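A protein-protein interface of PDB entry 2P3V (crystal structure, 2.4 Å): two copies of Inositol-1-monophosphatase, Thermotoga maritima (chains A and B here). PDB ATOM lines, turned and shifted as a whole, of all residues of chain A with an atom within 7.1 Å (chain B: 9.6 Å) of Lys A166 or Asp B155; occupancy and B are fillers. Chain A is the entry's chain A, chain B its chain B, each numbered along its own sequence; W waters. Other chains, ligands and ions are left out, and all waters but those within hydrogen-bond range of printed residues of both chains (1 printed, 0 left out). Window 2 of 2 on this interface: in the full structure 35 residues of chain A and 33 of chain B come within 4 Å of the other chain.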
ATOM      1  N   PHE A 160      38.042 -15.555 -14.876  1.00  0.00           N
ATOM      2  CA  PHE A 160      38.396 -16.524 -15.911  1.00  0.00           C
ATOM      3  C   PHE A 160      37.239 -16.609 -16.914  1.00  0.00           C
ATOM      4  O   PHE A 160      37.448 -16.640 -18.125  1.00  0.00           O
ATOM      5  CB  PHE A 160      38.669 -17.905 -15.288  1.00  0.00           C
ATOM      6  CG  PHE A 160      38.946 -18.986 -16.298  1.00  0.00           C
ATOM      7  CD1 PHE A 160      37.953 -19.893 -16.660  1.00  0.00           C
ATOM      8  CD2 PHE A 160      40.188 -19.073 -16.920  1.00  0.00           C
ATOM      9  CE1 PHE A 160      38.190 -20.872 -17.632  1.00  0.00           C
ATOM     10  CE2 PHE A 160      40.437 -20.050 -17.895  1.00  0.00           C
ATOM     11  CZ  PHE A 160      39.434 -20.949 -18.251  1.00  0.00           C
ATOM     12  N   ILE A 161      36.017 -16.640 -16.397  1.00  0.00           N
ATOM     13  CA  ILE A 161      34.832 -16.697 -17.240  1.00  0.00           C
ATOM     14  C   ILE A 161      34.681 -15.349 -17.923  1.00  0.00           C
ATOM     15  O   ILE A 161      34.164 -15.243 -19.037  1.00  0.00           O
ATOM     16  CB  ILE A 161      33.578 -16.955 -16.403  1.00  0.00           C
ATOM     17  CG1 ILE A 161      33.649 -18.351 -15.791  1.00  0.00           C
ATOM     18  CG2 ILE A 161      32.336 -16.784 -17.259  1.00  0.00           C
ATOM     19  CD1 ILE A 161      32.542 -18.636 -14.801  1.00  0.00           C
ATOM     20  N   GLU A 162      35.140 -14.319 -17.224  1.00  0.00           N
ATOM     21  CA  GLU A 162      35.087 -12.950 -17.708  1.00  0.00           C
ATOM     22  C   GLU A 162      35.810 -12.853 -19.047  1.00  0.00           C
ATOM     23  O   GLU A 162      35.261 -12.383 -20.041  1.00  0.00           O
ATOM     24  CB  GLU A 162      35.767 -12.027 -16.691  1.00  0.00           C
ATOM     25  CG  GLU A 162      35.587 -10.551 -16.971  1.00  0.00           C
ATOM     26  CD  GLU A 162      34.186 -10.076 -16.661  1.00  0.00           C
ATOM     27  OE1 GLU A 162      33.681  -9.193 -17.387  1.00  0.00           O
ATOM     28  OE2 GLU A 162      33.596 -10.578 -15.684  1.00  0.00           O
ATOM     29  N   ARG A 163      37.049 -13.322 -19.054  1.00  0.00           N
ATOM     30  CA  ARG A 163      37.892 -13.279 -20.233  1.00  0.00           C
ATOM     31  C   ARG A 163      37.598 -14.349 -21.269  1.00  0.00           C
ATOM     32  O   ARG A 163      37.796 -14.135 -22.466  1.00  0.00           O
ATOM     33  CB  ARG A 163      39.349 -13.384 -19.800  1.00  0.00           C
ATOM     34  CG  ARG A 163      39.820 -12.196 -18.991  1.00  0.00           C
ATOM     35  CD  ARG A 163      41.074 -12.528 -18.216  1.00  0.00           C
ATOM     36  NE  ARG A 163      41.940 -11.366 -18.077  1.00  0.00           N
ATOM     37  CZ  ARG A 163      42.579 -10.793 -19.091  1.00  0.00           C
ATOM     38  NH1 ARG A 163      43.350  -9.736 -18.877  1.00  0.00           N
ATOM     39  NH2 ARG A 163      42.452 -11.282 -20.320  1.00  0.00           N
ATOM     40  N   MET A 164      37.111 -15.494 -20.812  1.00  0.00           N
ATOM     41  CA  MET A 164      36.843 -16.611 -21.705  1.00  0.00           C
ATOM     42  C   MET A 164      35.490 -16.592 -22.406  1.00  0.00           C
ATOM     43  O   MET A 164      35.406 -16.853 -23.601  1.00  0.00           O
ATOM     44  CB  MET A 164      37.001 -17.922 -20.934  1.00  0.00           C
ATOM     45  CG  MET A 164      37.277 -19.126 -21.810  1.00  0.00           C
ATOM     46  SD  MET A 164      38.869 -19.030 -22.674  1.00  0.00           S
ATOM     47  CE  MET A 164      39.932 -19.969 -21.557  1.00  0.00           C
ATOM     48  N   GLU A 165      34.434 -16.290 -21.664  1.00  0.00           N
ATOM     49  CA  GLU A 165      33.086 -16.266 -22.225  1.00  0.00           C
ATOM     50  C   GLU A 165      33.033 -15.449 -23.517  1.00  0.00           C
ATOM     51  O   GLU A 165      32.183 -15.679 -24.378  1.00  0.00           O
ATOM     52  CB  GLU A 165      32.110 -15.694 -21.186  1.00  0.00           C
ATOM     53  CG  GLU A 165      30.658 -16.164 -21.318  1.00  0.00           C
ATOM     54  CD  GLU A 165      30.512 -17.684 -21.316  1.00  0.00           C
ATOM     55  OE1 GLU A 165      30.843 -18.318 -22.341  1.00  0.00           O
ATOM     56  OE2 GLU A 165      30.072 -18.247 -20.287  1.00  0.00           O
ATOM     57  N   LYS A 166      33.961 -14.508 -23.659  1.00  0.00           N
ATOM     58  CA  LYS A 166      34.014 -13.661 -24.841  1.00  0.00           C
ATOM     59  C   LYS A 166      34.486 -14.402 -26.088  1.00  0.00           C
ATOM     60  O   LYS A 166      34.016 -14.129 -27.192  1.00  0.00           O
ATOM     61  CB  LYS A 166      34.950 -12.475 -24.599  1.00  0.00           C
ATOM     62  CG  LYS A 166      34.722 -11.759 -23.285  1.00  0.00           C
ATOM     63  CD  LYS A 166      35.527 -10.470 -23.212  1.00  0.00           C
ATOM     64  CE  LYS A 166      35.485  -9.850 -21.811  1.00  0.00           C
ATOM     65  NZ  LYS A 166      34.100  -9.554 -21.323  1.00  0.00           N
ATOM     66  N   ARG A 167      35.409 -15.344 -25.918  1.00  0.00           N
ATOM     67  CA  ARG A 167      35.961 -16.063 -27.062  1.00  0.00           C
ATOM     68  C   ARG A 167      35.575 -17.527 -27.262  1.00  0.00           C
ATOM     69  O   ARG A 167      36.145 -18.205 -28.116  1.00  0.00           O
ATOM     70  CB  ARG A 167      37.488 -15.912 -27.064  1.00  0.00           C
ATOM     71  CG  ARG A 167      38.082 -15.570 -25.706  1.00  0.00           C
ATOM     72  CD  ARG A 167      39.404 -14.821 -25.823  1.00  0.00           C
ATOM     73  NE  ARG A 167      40.379 -15.526 -26.650  1.00  0.00           N
ATOM     74  CZ  ARG A 167      41.691 -15.292 -26.632  1.00  0.00           C
ATOM     75  NH1 ARG A 167      42.198 -14.365 -25.826  1.00  0.00           N
ATOM     76  NH2 ARG A 167      42.505 -15.999 -27.411  1.00  0.00           N
ATOM     77  N   THR A 168      34.597 -18.012 -26.501  1.00  0.00           N
ATOM     78  CA  THR A 168      34.153 -19.397 -26.646  1.00  0.00           C
ATOM     79  C   THR A 168      32.641 -19.467 -26.717  1.00  0.00           C
ATOM     80  O   THR A 168      31.965 -18.446 -26.611  1.00  0.00           O
ATOM     81  CB  THR A 168      34.621 -20.285 -25.464  1.00  0.00           C
ATOM     82  OG1 THR A 168      34.118 -19.759 -24.229  1.00  0.00           O
ATOM     83  CG2 THR A 168      36.126 -20.342 -25.413  1.00  0.00           C
ATOM     84  N   ARG A 169      32.112 -20.671 -26.912  1.00  0.00           N
ATOM     85  CA  ARG A 169      30.667 -20.853 -26.962  1.00  0.00           C
ATOM     86  C   ARG A 169      30.078 -20.695 -25.567  1.00  0.00           C
ATOM     87  O   ARG A 169      29.186 -19.876 -25.347  1.00  0.00           O
ATOM     88  CB  ARG A 169      30.315 -22.238 -27.484  1.00  0.00           C
ATOM     89  CG  ARG A 169      30.456 -22.369 -28.961  1.00  0.00           C
ATOM     90  CD  ARG A 169      29.980 -23.716 -29.425  1.00  0.00           C
ATOM     91  NE  ARG A 169      29.944 -23.772 -30.879  1.00  0.00           N
ATOM     92  CZ  ARG A 169      29.913 -24.900 -31.573  1.00  0.00           C
ATOM     93  NH1 ARG A 169      29.914 -26.065 -30.934  1.00  0.00           N
ATOM     94  NH2 ARG A 169      29.886 -24.864 -32.900  1.00  0.00           N
ATOM     95  N   ILE A 171      31.060 -21.604 -21.024  1.00  0.00           N
ATOM     96  CA  ILE A 171      32.009 -22.108 -20.048  1.00  0.00           C
ATOM     97  C   ILE A 171      31.126 -22.693 -18.965  1.00  0.00           C
ATOM     98  O   ILE A 171      30.242 -22.017 -18.432  1.00  0.00           O
ATOM     99  CB  ILE A 171      32.942 -21.019 -19.478  1.00  0.00           C
ATOM    100  CG1 ILE A 171      33.811 -20.429 -20.600  1.00  0.00           C
ATOM    101  CG2 ILE A 171      33.869 -21.635 -18.430  1.00  0.00           C
ATOM    102  CD1 ILE A 171      34.765 -21.430 -21.259  1.00  0.00           C
ATOM    103  N   PHE B  34      28.292 -16.962 -32.868  1.00  0.00           N
ATOM    104  CA  PHE B  34      28.832 -18.305 -32.641  1.00  0.00           C
ATOM    105  C   PHE B  34      28.427 -18.875 -31.281  1.00  0.00           C
ATOM    106  O   PHE B  34      28.540 -20.081 -31.037  1.00  0.00           O
ATOM    107  CB  PHE B  34      30.367 -18.344 -32.821  1.00  0.00           C
ATOM    108  CG  PHE B  34      31.145 -17.552 -31.800  1.00  0.00           C
ATOM    109  CD1 PHE B  34      31.822 -16.395 -32.174  1.00  0.00           C
ATOM    110  CD2 PHE B  34      31.254 -17.994 -30.481  1.00  0.00           C
ATOM    111  CE1 PHE B  34      32.601 -15.688 -31.249  1.00  0.00           C
ATOM    112  CE2 PHE B  34      32.030 -17.297 -29.549  1.00  0.00           C
ATOM    113  CZ  PHE B  34      32.704 -16.142 -29.934  1.00  0.00           C
ATOM    114  N   LYS B  35      27.943 -18.004 -30.405  1.00  0.00           N
ATOM    115  CA  LYS B  35      27.494 -18.427 -29.091  1.00  0.00           C
ATOM    116  C   LYS B  35      26.007 -18.777 -29.144  1.00  0.00           C
ATOM    117  O   LYS B  35      25.477 -19.376 -28.213  1.00  0.00           O
ATOM    118  CB  LYS B  35      27.743 -17.315 -28.065  1.00  0.00           C
ATOM    119  CG  LYS B  35      29.213 -17.024 -27.842  1.00  0.00           C
ATOM    120  CD  LYS B  35      29.441 -15.918 -26.819  1.00  0.00           C
ATOM    121  CE  LYS B  35      29.192 -16.386 -25.387  1.00  0.00           C
ATOM    122  NZ  LYS B  35      30.267 -17.286 -24.875  1.00  0.00           N
ATOM    123  N   GLY B 151      23.060 -18.731 -15.999  1.00  0.00           N
ATOM    124  CA  GLY B 151      23.399 -19.059 -17.371  1.00  0.00           C
ATOM    125  C   GLY B 151      24.709 -18.425 -17.799  1.00  0.00           C
ATOM    126  O   GLY B 151      25.361 -17.746 -17.012  1.00  0.00           O
ATOM    127  N   SER B 152      25.100 -18.641 -19.050  1.00  0.00           N
ATOM    128  CA  SER B 152      26.346 -18.086 -19.568  1.00  0.00           C
ATOM    129  C   SER B 152      26.104 -16.871 -20.456  1.00  0.00           C
ATOM    130  O   SER B 152      26.021 -16.974 -21.682  1.00  0.00           O
ATOM    131  CB  SER B 152      27.126 -19.153 -20.346  1.00  0.00           C
ATOM    132  OG  SER B 152      27.607 -20.174 -19.485  1.00  0.00           O
ATOM    133  N   TYR B 153      25.993 -15.718 -19.812  1.00  0.00           N
ATOM    134  CA  TYR B 153      25.767 -14.455 -20.497  1.00  0.00           C
ATOM    135  C   TYR B 153      27.071 -13.655 -20.447  1.00  0.00           C
ATOM    136  O   TYR B 153      27.656 -13.475 -19.378  1.00  0.00           O
ATOM    137  CB  TYR B 153      24.653 -13.683 -19.786  1.00  0.00           C
ATOM    138  CG  TYR B 153      23.517 -14.567 -19.307  1.00  0.00           C
ATOM    139  CD1 TYR B 153      22.692 -15.231 -20.215  1.00  0.00           C
ATOM    140  CD2 TYR B 153      23.286 -14.761 -17.941  1.00  0.00           C
ATOM    141  CE1 TYR B 153      21.667 -16.069 -19.778  1.00  0.00           C
ATOM    142  CE2 TYR B 153      22.264 -15.597 -17.492  1.00  0.00           C
ATOM    143  CZ  TYR B 153      21.460 -16.247 -18.415  1.00  0.00           C
ATOM    144  OH  TYR B 153      20.457 -17.083 -17.987  1.00  0.00           O
ATOM    145  N   VAL B 154      27.534 -13.187 -21.599  1.00  0.00           N
ATOM    146  CA  VAL B 154      28.767 -12.417 -21.633  1.00  0.00           C
ATOM    147  C   VAL B 154      28.606 -11.163 -20.769  1.00  0.00           C
ATOM    148  O   VAL B 154      27.543 -10.536 -20.750  1.00  0.00           O
ATOM    149  CB  VAL B 154      29.141 -12.029 -23.082  1.00  0.00           C
ATOM    150  CG1 VAL B 154      28.050 -11.169 -23.695  1.00  0.00           C
ATOM    151  CG2 VAL B 154      30.473 -11.318 -23.093  1.00  0.00           C
ATOM    152  N   ASP B 155      29.664 -10.832 -20.034  1.00  0.00           N
ATOM    153  CA  ASP B 155      29.702  -9.671 -19.139  1.00  0.00           C
ATOM    154  C   ASP B 155      28.976  -9.855 -17.806  1.00  0.00           C
ATOM    155  O   ASP B 155      29.544  -9.579 -16.748  1.00  0.00           O
ATOM    156  CB  ASP B 155      29.178  -8.410 -19.848  1.00  0.00           C
ATOM    157  CG  ASP B 155      30.177  -7.849 -20.865  1.00  0.00           C
ATOM    158  OD1 ASP B 155      31.369  -7.686 -20.509  1.00  0.00           O
ATOM    159  OD2 ASP B 155      29.771  -7.563 -22.017  1.00  0.00           O
ATOM    160  N   PHE B 156      27.738 -10.327 -17.846  1.00  0.00           N
ATOM    161  CA  PHE B 156      26.987 -10.526 -16.610  1.00  0.00           C
ATOM    162  C   PHE B 156      27.466 -11.706 -15.763  1.00  0.00           C
ATOM    163  O   PHE B 156      27.506 -11.615 -14.537  1.00  0.00           O
ATOM    164  CB  PHE B 156      25.491 -10.700 -16.917  1.00  0.00           C
ATOM    165  CG  PHE B 156      24.651 -11.038 -15.706  1.00  0.00           C
ATOM    166  CD1 PHE B 156      24.597 -12.343 -15.211  1.00  0.00           C
ATOM    167  CD2 PHE B 156      23.936 -10.044 -15.038  1.00  0.00           C
ATOM    168  CE1 PHE B 156      23.844 -12.652 -14.070  1.00  0.00           C
ATOM    169  CE2 PHE B 156      23.181 -10.344 -13.898  1.00  0.00           C
ATOM    170  CZ  PHE B 156      23.140 -11.650 -13.415  1.00  0.00           C
ATOM    171  N   THR B 157      27.824 -12.809 -16.413  1.00  0.00           N
ATOM    172  CA  THR B 157      28.253 -14.000 -15.685  1.00  0.00           C
ATOM    173  C   THR B 157      29.484 -13.773 -14.831  1.00  0.00           C
ATOM    174  O   THR B 157      29.424 -13.901 -13.607  1.00  0.00           O
ATOM    175  CB  THR B 157      28.539 -15.179 -16.629  1.00  0.00           C
ATOM    176  OG1 THR B 157      27.375 -15.461 -17.414  1.00  0.00           O
ATOM    177  CG2 THR B 157      28.882 -16.415 -15.822  1.00  0.00           C
ATOM    178  N   GLY B 158      30.601 -13.452 -15.475  1.00  0.00           N
ATOM    179  CA  GLY B 158      31.826 -13.213 -14.739  1.00  0.00           C
ATOM    180  C   GLY B 158      31.583 -12.322 -13.537  1.00  0.00           C
ATOM    181  O   GLY B 158      32.096 -12.586 -12.450  1.00  0.00           O
ATOM    182  N   LYS B 159      30.790 -11.271 -13.729  1.00  0.00           N
ATOM    183  CA  LYS B 159      30.480 -10.338 -12.654  1.00  0.00           C
ATOM    184  C   LYS B 159      29.654 -10.977 -11.542  1.00  0.00           C
ATOM    185  O   LYS B 159      29.931 -10.772 -10.361  1.00  0.00           O
ATOM    186  CB  LYS B 159      29.737  -9.121 -13.211  1.00  0.00           C
ATOM    187  CG  LYS B 159      30.624  -8.154 -13.984  1.00  0.00           C
ATOM    188  CD  LYS B 159      31.611  -7.450 -13.050  1.00  0.00           C
ATOM    189  CE  LYS B 159      32.535  -6.481 -13.803  1.00  0.00           C
ATOM    190  NZ  LYS B 159      33.426  -5.675 -12.893  1.00  0.00           N
ATOM    191  N   PHE B 160      28.645 -11.755 -11.925  1.00  0.00           N
ATOM    192  CA  PHE B 160      27.770 -12.411 -10.957  1.00  0.00           C
ATOM    193  C   PHE B 160      28.532 -13.357 -10.041  1.00  0.00           C
ATOM    194  O   PHE B 160      28.338 -13.341  -8.825  1.00  0.00           O
ATOM    195  CB  PHE B 160      26.653 -13.171 -11.687  1.00  0.00           C
ATOM    196  CG  PHE B 160      25.630 -13.795 -10.764  1.00  0.00           C
ATOM    197  CD1 PHE B 160      25.698 -15.151 -10.437  1.00  0.00           C
ATOM    198  CD2 PHE B 160      24.594 -13.028 -10.228  1.00  0.00           C
ATOM    199  CE1 PHE B 160      24.748 -15.732  -9.598  1.00  0.00           C
ATOM    200  CE2 PHE B 160      23.638 -13.604  -9.384  1.00  0.00           C
ATOM    201  CZ  PHE B 160      23.715 -14.957  -9.072  1.00  0.00           C
ATOM    202  N   ILE B 161      29.386 -14.187 -10.631  1.00  0.00           N
ATOM    203  CA  ILE B 161      30.176 -15.132  -9.858  1.00  0.00           C
ATOM    204  C   ILE B 161      31.024 -14.319  -8.908  1.00  0.00           C
ATOM    205  O   ILE B 161      31.007 -14.532  -7.701  1.00  0.00           O
ATOM    206  CB  ILE B 161      31.123 -15.973 -10.761  1.00  0.00           C
ATOM    207  CG1 ILE B 161      30.380 -17.176 -11.338  1.00  0.00           C
ATOM    208  CG2 ILE B 161      32.333 -16.444  -9.969  1.00  0.00           C
ATOM    209  CD1 ILE B 161      29.339 -16.822 -12.352  1.00  0.00           C
ATOM    210  N   GLU B 162      31.761 -13.383  -9.485  1.00  0.00           N
ATOM    211  CA  GLU B 162      32.657 -12.495  -8.757  1.00  0.00           C
ATOM    212  C   GLU B 162      32.050 -11.976  -7.456  1.00  0.00           C
ATOM    213  O   GLU B 162      32.698 -11.964  -6.410  1.00  0.00           O
ATOM    214  CB  GLU B 162      33.014 -11.329  -9.674  1.00  0.00           C
ATOM    215  CG  GLU B 162      34.076 -10.386  -9.172  1.00  0.00           C
ATOM    216  CD  GLU B 162      34.386  -9.322 -10.209  1.00  0.00           C
ATOM    217  OE1 GLU B 162      34.851  -9.686 -11.315  1.00  0.00           O
ATOM    218  OE2 GLU B 162      34.153  -8.126  -9.923  1.00  0.00           O
ATOM    219  N   ARG B 163      30.793 -11.557  -7.535  1.00  0.00           N
ATOM    220  CA  ARG B 163      30.084 -11.021  -6.385  1.00  0.00           C
ATOM    221  C   ARG B 163      29.565 -12.134  -5.479  1.00  0.00           C
ATOM    222  O   ARG B 163      29.858 -12.179  -4.281  1.00  0.00           O
ATOM    223  CB  ARG B 163      28.910 -10.165  -6.869  1.00  0.00           C
ATOM    224  CG  ARG B 163      28.405  -9.151  -5.854  1.00  0.00           C
ATOM    225  CD  ARG B 163      28.048  -9.803  -4.519  1.00  0.00           C
ATOM    226  NE  ARG B 163      27.639  -8.827  -3.511  1.00  0.00           N
ATOM    227  CZ  ARG B 163      27.306  -9.136  -2.261  1.00  0.00           C
ATOM    228  NH1 ARG B 163      27.333 -10.401  -1.854  1.00  0.00           N
ATOM    229  NH2 ARG B 163      26.943  -8.177  -1.416  1.00  0.00           N
ATOM    230  N   TRP B 195      19.384 -13.888 -17.174  1.00  0.00           N
ATOM    231  CA  TRP B 195      19.585 -12.566 -17.767  1.00  0.00           C
ATOM    232  C   TRP B 195      19.143 -12.674 -19.231  1.00  0.00           C
ATOM    233  O   TRP B 195      19.645 -13.533 -19.955  1.00  0.00           O
ATOM    234  CB  TRP B 195      21.083 -12.248 -17.677  1.00  0.00           C
ATOM    235  CG  TRP B 195      21.563 -10.909 -18.157  1.00  0.00           C
ATOM    236  CD1 TRP B 195      22.691 -10.673 -18.892  1.00  0.00           C
ATOM    237  CD2 TRP B 195      21.024  -9.621 -17.833  1.00  0.00           C
ATOM    238  NE1 TRP B 195      22.897  -9.326 -19.035  1.00  0.00           N
ATOM    239  CE2 TRP B 195      21.895  -8.653 -18.390  1.00  0.00           C
ATOM    240  CE3 TRP B 195      19.905  -9.186 -17.110  1.00  0.00           C
ATOM    241  CZ2 TRP B 195      21.669  -7.278 -18.264  1.00  0.00           C
ATOM    242  CZ3 TRP B 195      19.682  -7.813 -16.983  1.00  0.00           C
ATOM    243  CH2 TRP B 195      20.568  -6.878 -17.552  1.00  0.00           C
ATOM    244  N   ARG B 196      18.217 -11.825 -19.675  1.00  0.00           N
ATOM    245  CA  ARG B 196      17.752 -11.896 -21.069  1.00  0.00           C
ATOM    246  C   ARG B 196      17.172 -13.285 -21.311  1.00  0.00           C
ATOM    247  O   ARG B 196      17.922 -14.252 -21.396  1.00  0.00           O
ATOM    248  CB  ARG B 196      18.914 -11.690 -22.057  1.00  0.00           C
ATOM    249  CG  ARG B 196      19.359 -10.253 -22.293  1.00  0.00           C
ATOM    250  CD  ARG B 196      20.812 -10.056 -21.885  1.00  0.00           C
ATOM    251  NE  ARG B 196      21.498  -9.021 -22.661  1.00  0.00           N
ATOM    252  CZ  ARG B 196      21.188  -7.724 -22.670  1.00  0.00           C
ATOM    253  NH1 ARG B 196      21.894  -6.893 -23.421  1.00  0.00           N
ATOM    254  NH2 ARG B 196      20.188  -7.250 -21.942  1.00  0.00           N
ATOM    255  N   VAL B 249      25.206  -6.298  -9.344  1.00  0.00           N
ATOM    256  CA  VAL B 249      25.858  -6.726 -10.575  1.00  0.00           C
ATOM    257  C   VAL B 249      25.353  -5.980 -11.809  1.00  0.00           C
ATOM    258  O   VAL B 249      26.142  -5.458 -12.597  1.00  0.00           O
ATOM    259  CB  VAL B 249      25.641  -8.239 -10.813  1.00  0.00           C
ATOM    260  CG1 VAL B 249      26.382  -8.683 -12.071  1.00  0.00           C
ATOM    261  CG2 VAL B 249      26.102  -9.029  -9.596  1.00  0.00           C
ATOM    262  N   VAL B 250      24.035  -5.935 -11.977  1.00  0.00           N
ATOM    263  CA  VAL B 250      23.454  -5.275 -13.133  1.00  0.00           C
ATOM    264  C   VAL B 250      23.740  -3.775 -13.169  1.00  0.00           C
ATOM    265  O   VAL B 250      23.845  -3.181 -14.246  1.00  0.00           O
ATOM    266  CB  VAL B 250      21.933  -5.512 -13.199  1.00  0.00           C
ATOM    267  CG1 VAL B 250      21.251  -4.859 -12.012  1.00  0.00           C
ATOM    268  CG2 VAL B 250      21.383  -4.976 -14.518  1.00  0.00           C
ATOM    269  N   GLU B 252      26.442  -2.483 -11.588  1.00  0.00           N
ATOM    270  CA  GLU B 252      27.890  -2.453 -11.734  1.00  0.00           C
ATOM    271  C   GLU B 252      28.200  -2.498 -13.221  1.00  0.00           C
ATOM    272  O   GLU B 252      29.309  -2.176 -13.641  1.00  0.00           O
ATOM    273  CB  GLU B 252      28.534  -3.652 -11.035  1.00  0.00           C
ATOM    274  CG  GLU B 252      30.059  -3.661 -11.103  1.00  0.00           C
ATOM    275  CD  GLU B 252      30.683  -4.868 -10.412  1.00  0.00           C
ATOM    276  OE1 GLU B 252      31.928  -4.970 -10.403  1.00  0.00           O
ATOM    277  OE2 GLU B 252      29.934  -5.715  -9.878  1.00  0.00           O
ATOM    278  N   ILE B 253      27.213  -2.912 -14.012  1.00  0.00           N
ATOM    279  CA  ILE B 253      27.367  -2.970 -15.462  1.00  0.00           C
ATOM    280  C   ILE B 253      26.718  -1.717 -16.050  1.00  0.00           C
ATOM    281  O   ILE B 253      27.234  -0.607 -15.900  1.00  0.00           O
ATOM    282  CB  ILE B 253      26.671  -4.210 -16.084  1.00  0.00           C
ATOM    283  CG1 ILE B 253      27.170  -5.497 -15.425  1.00  0.00           C
ATOM    284  CG2 ILE B 253      26.958  -4.268 -17.583  1.00  0.00           C
ATOM    285  CD1 ILE B 253      26.464  -6.756 -15.937  1.00  0.00           C
ATOM    286  N   GLY B 254      25.573  -1.903 -16.698  1.00  0.00           N
ATOM    287  CA  GLY B 254      24.880  -0.785 -17.303  1.00  0.00           C
ATOM    288  C   GLY B 254      25.551  -0.408 -18.607  1.00  0.00           C
ATOM    289  O   GLY B 254      26.463  -1.148 -19.036  1.00  0.00           O
HETATM  290  O   HOH W   1      32.300 -11.876 -20.303  1.00  0.00           O
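4 positions are printed for both chains.
The side-chain carboxylate of Glu A162 sits at hydrogen-bond distance from the backbone NH of Lys B159, at 3.5 Å. The side-chain amino group (NZ) of Lys B35 is in salt-bridge range of the side-chain carboxylate (OE1) of Glu A165 (2.8 Å). The side-chain hydroxyl (OG) of Ser B152 lies close to the side-chain carboxylate (OE2) of Glu A165 (3.2 Å). The side-chain carboxylate of Asp B155 is in salt-bridge range of the side-chain amino group of Lys A166 (3.4 Å). The backbone carbonyl oxygen of Thr A168 lies within hydrogen-bond range of the side-chain amino group of Lys B35. The side-chain amino group (NZ) of Lys B35 sits at hydrogen-bond distance from the backbone carbonyl oxygen (O) of Arg A169 (2.8 Å). The backbone carbonyl oxygen (O) of Ile A171 sits at hydrogen-bond distance from the side-chain hydroxyl (OG) of Ser B152 (3.4 Å).
NZ of Lys A166 lies within salt-bridge range of OE1 of Glu A162 (3.97 Å). The side-chain hydroxyl (OG1) of Thr A168 is in hydrogen-bond range of the backbone carbonyl oxygen (O) of Met A164. OG1 of Thr B157 lies within hydrogen-bond range of O of Gly B151, 3.1 Å away. The side-chain hydroxyl (OG1) of Thr B157 lies within hydrogen-bond range of the backbone NH (N) of Tyr B153 (2.8 Å). The side-chain amino group of Lys B159 is in salt-bridge range of the side-chain carboxylate of Glu B162. NZ of Lys B159 lies within salt-bridge range of OE1 of Glu B252 (3.0 Å).
Of the 11 printed residues of chain A, 7 touch a printed residue of chain B. Printed residues of chain A that touch a printed residue of chain B: Ile A161, Glu A162, Glu A165, Lys A166, Thr A168, Arg A169 and Ile A171. Along chain A the printed residues that touch a printed residue of chain B span positions 161 to 171. Hydrophobic or aromatic side chains of chain B within 4 Å of the printed part of chain A: Phe B34. Along chain B the printed residues that touch a printed residue of chain A span positions 34 to 159. Among the printed residues, 12 pairs touch across the chains.
Printed residues of chain B within 4 Å of Glu A165: Lys B35 (2.5 Å) and Ser B152 (3.1 Å). Of the printed residues of chain B, Arg A169 touches Phe B34 and Lys B35. Printed residues of chain B within 4 Å of Ile A171: Ser B152 (3.4 Å). Of chain A, only Lys A166 (3.4 Å) comes within 4 Å of Asp B155. The nearest residue of chain B that does not touch Lys A166 is Val B154 (4.3 Å). The nearest residue of chain A that does not touch Asp B155 is Glu A162 (4.2 Å). The nearest printed residue of chain B that does not touch Ile A171 is Lys B35 (5.8 Å).
CG2 of Thr B157 touches CG2 of Ile A161, at 3.8 Å. OE2 of Glu A162 touches CA of Gly B158 (3.3 Å). O of Lys A166 touches CZ of Phe B34, 3.6 Å away. O of Thr A168 touches CE2 of Phe B34 (3.2 Å). O of Phe B34 touches CG of Arg A169, at 3.6 Å.
Water W1 lies within hydrogen-bond range of the backbone NH (N) of Asp B155, the backbone carbonyl oxygen (O) of Glu A162 and the side-chain amino group (NZ) of Lys A166.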
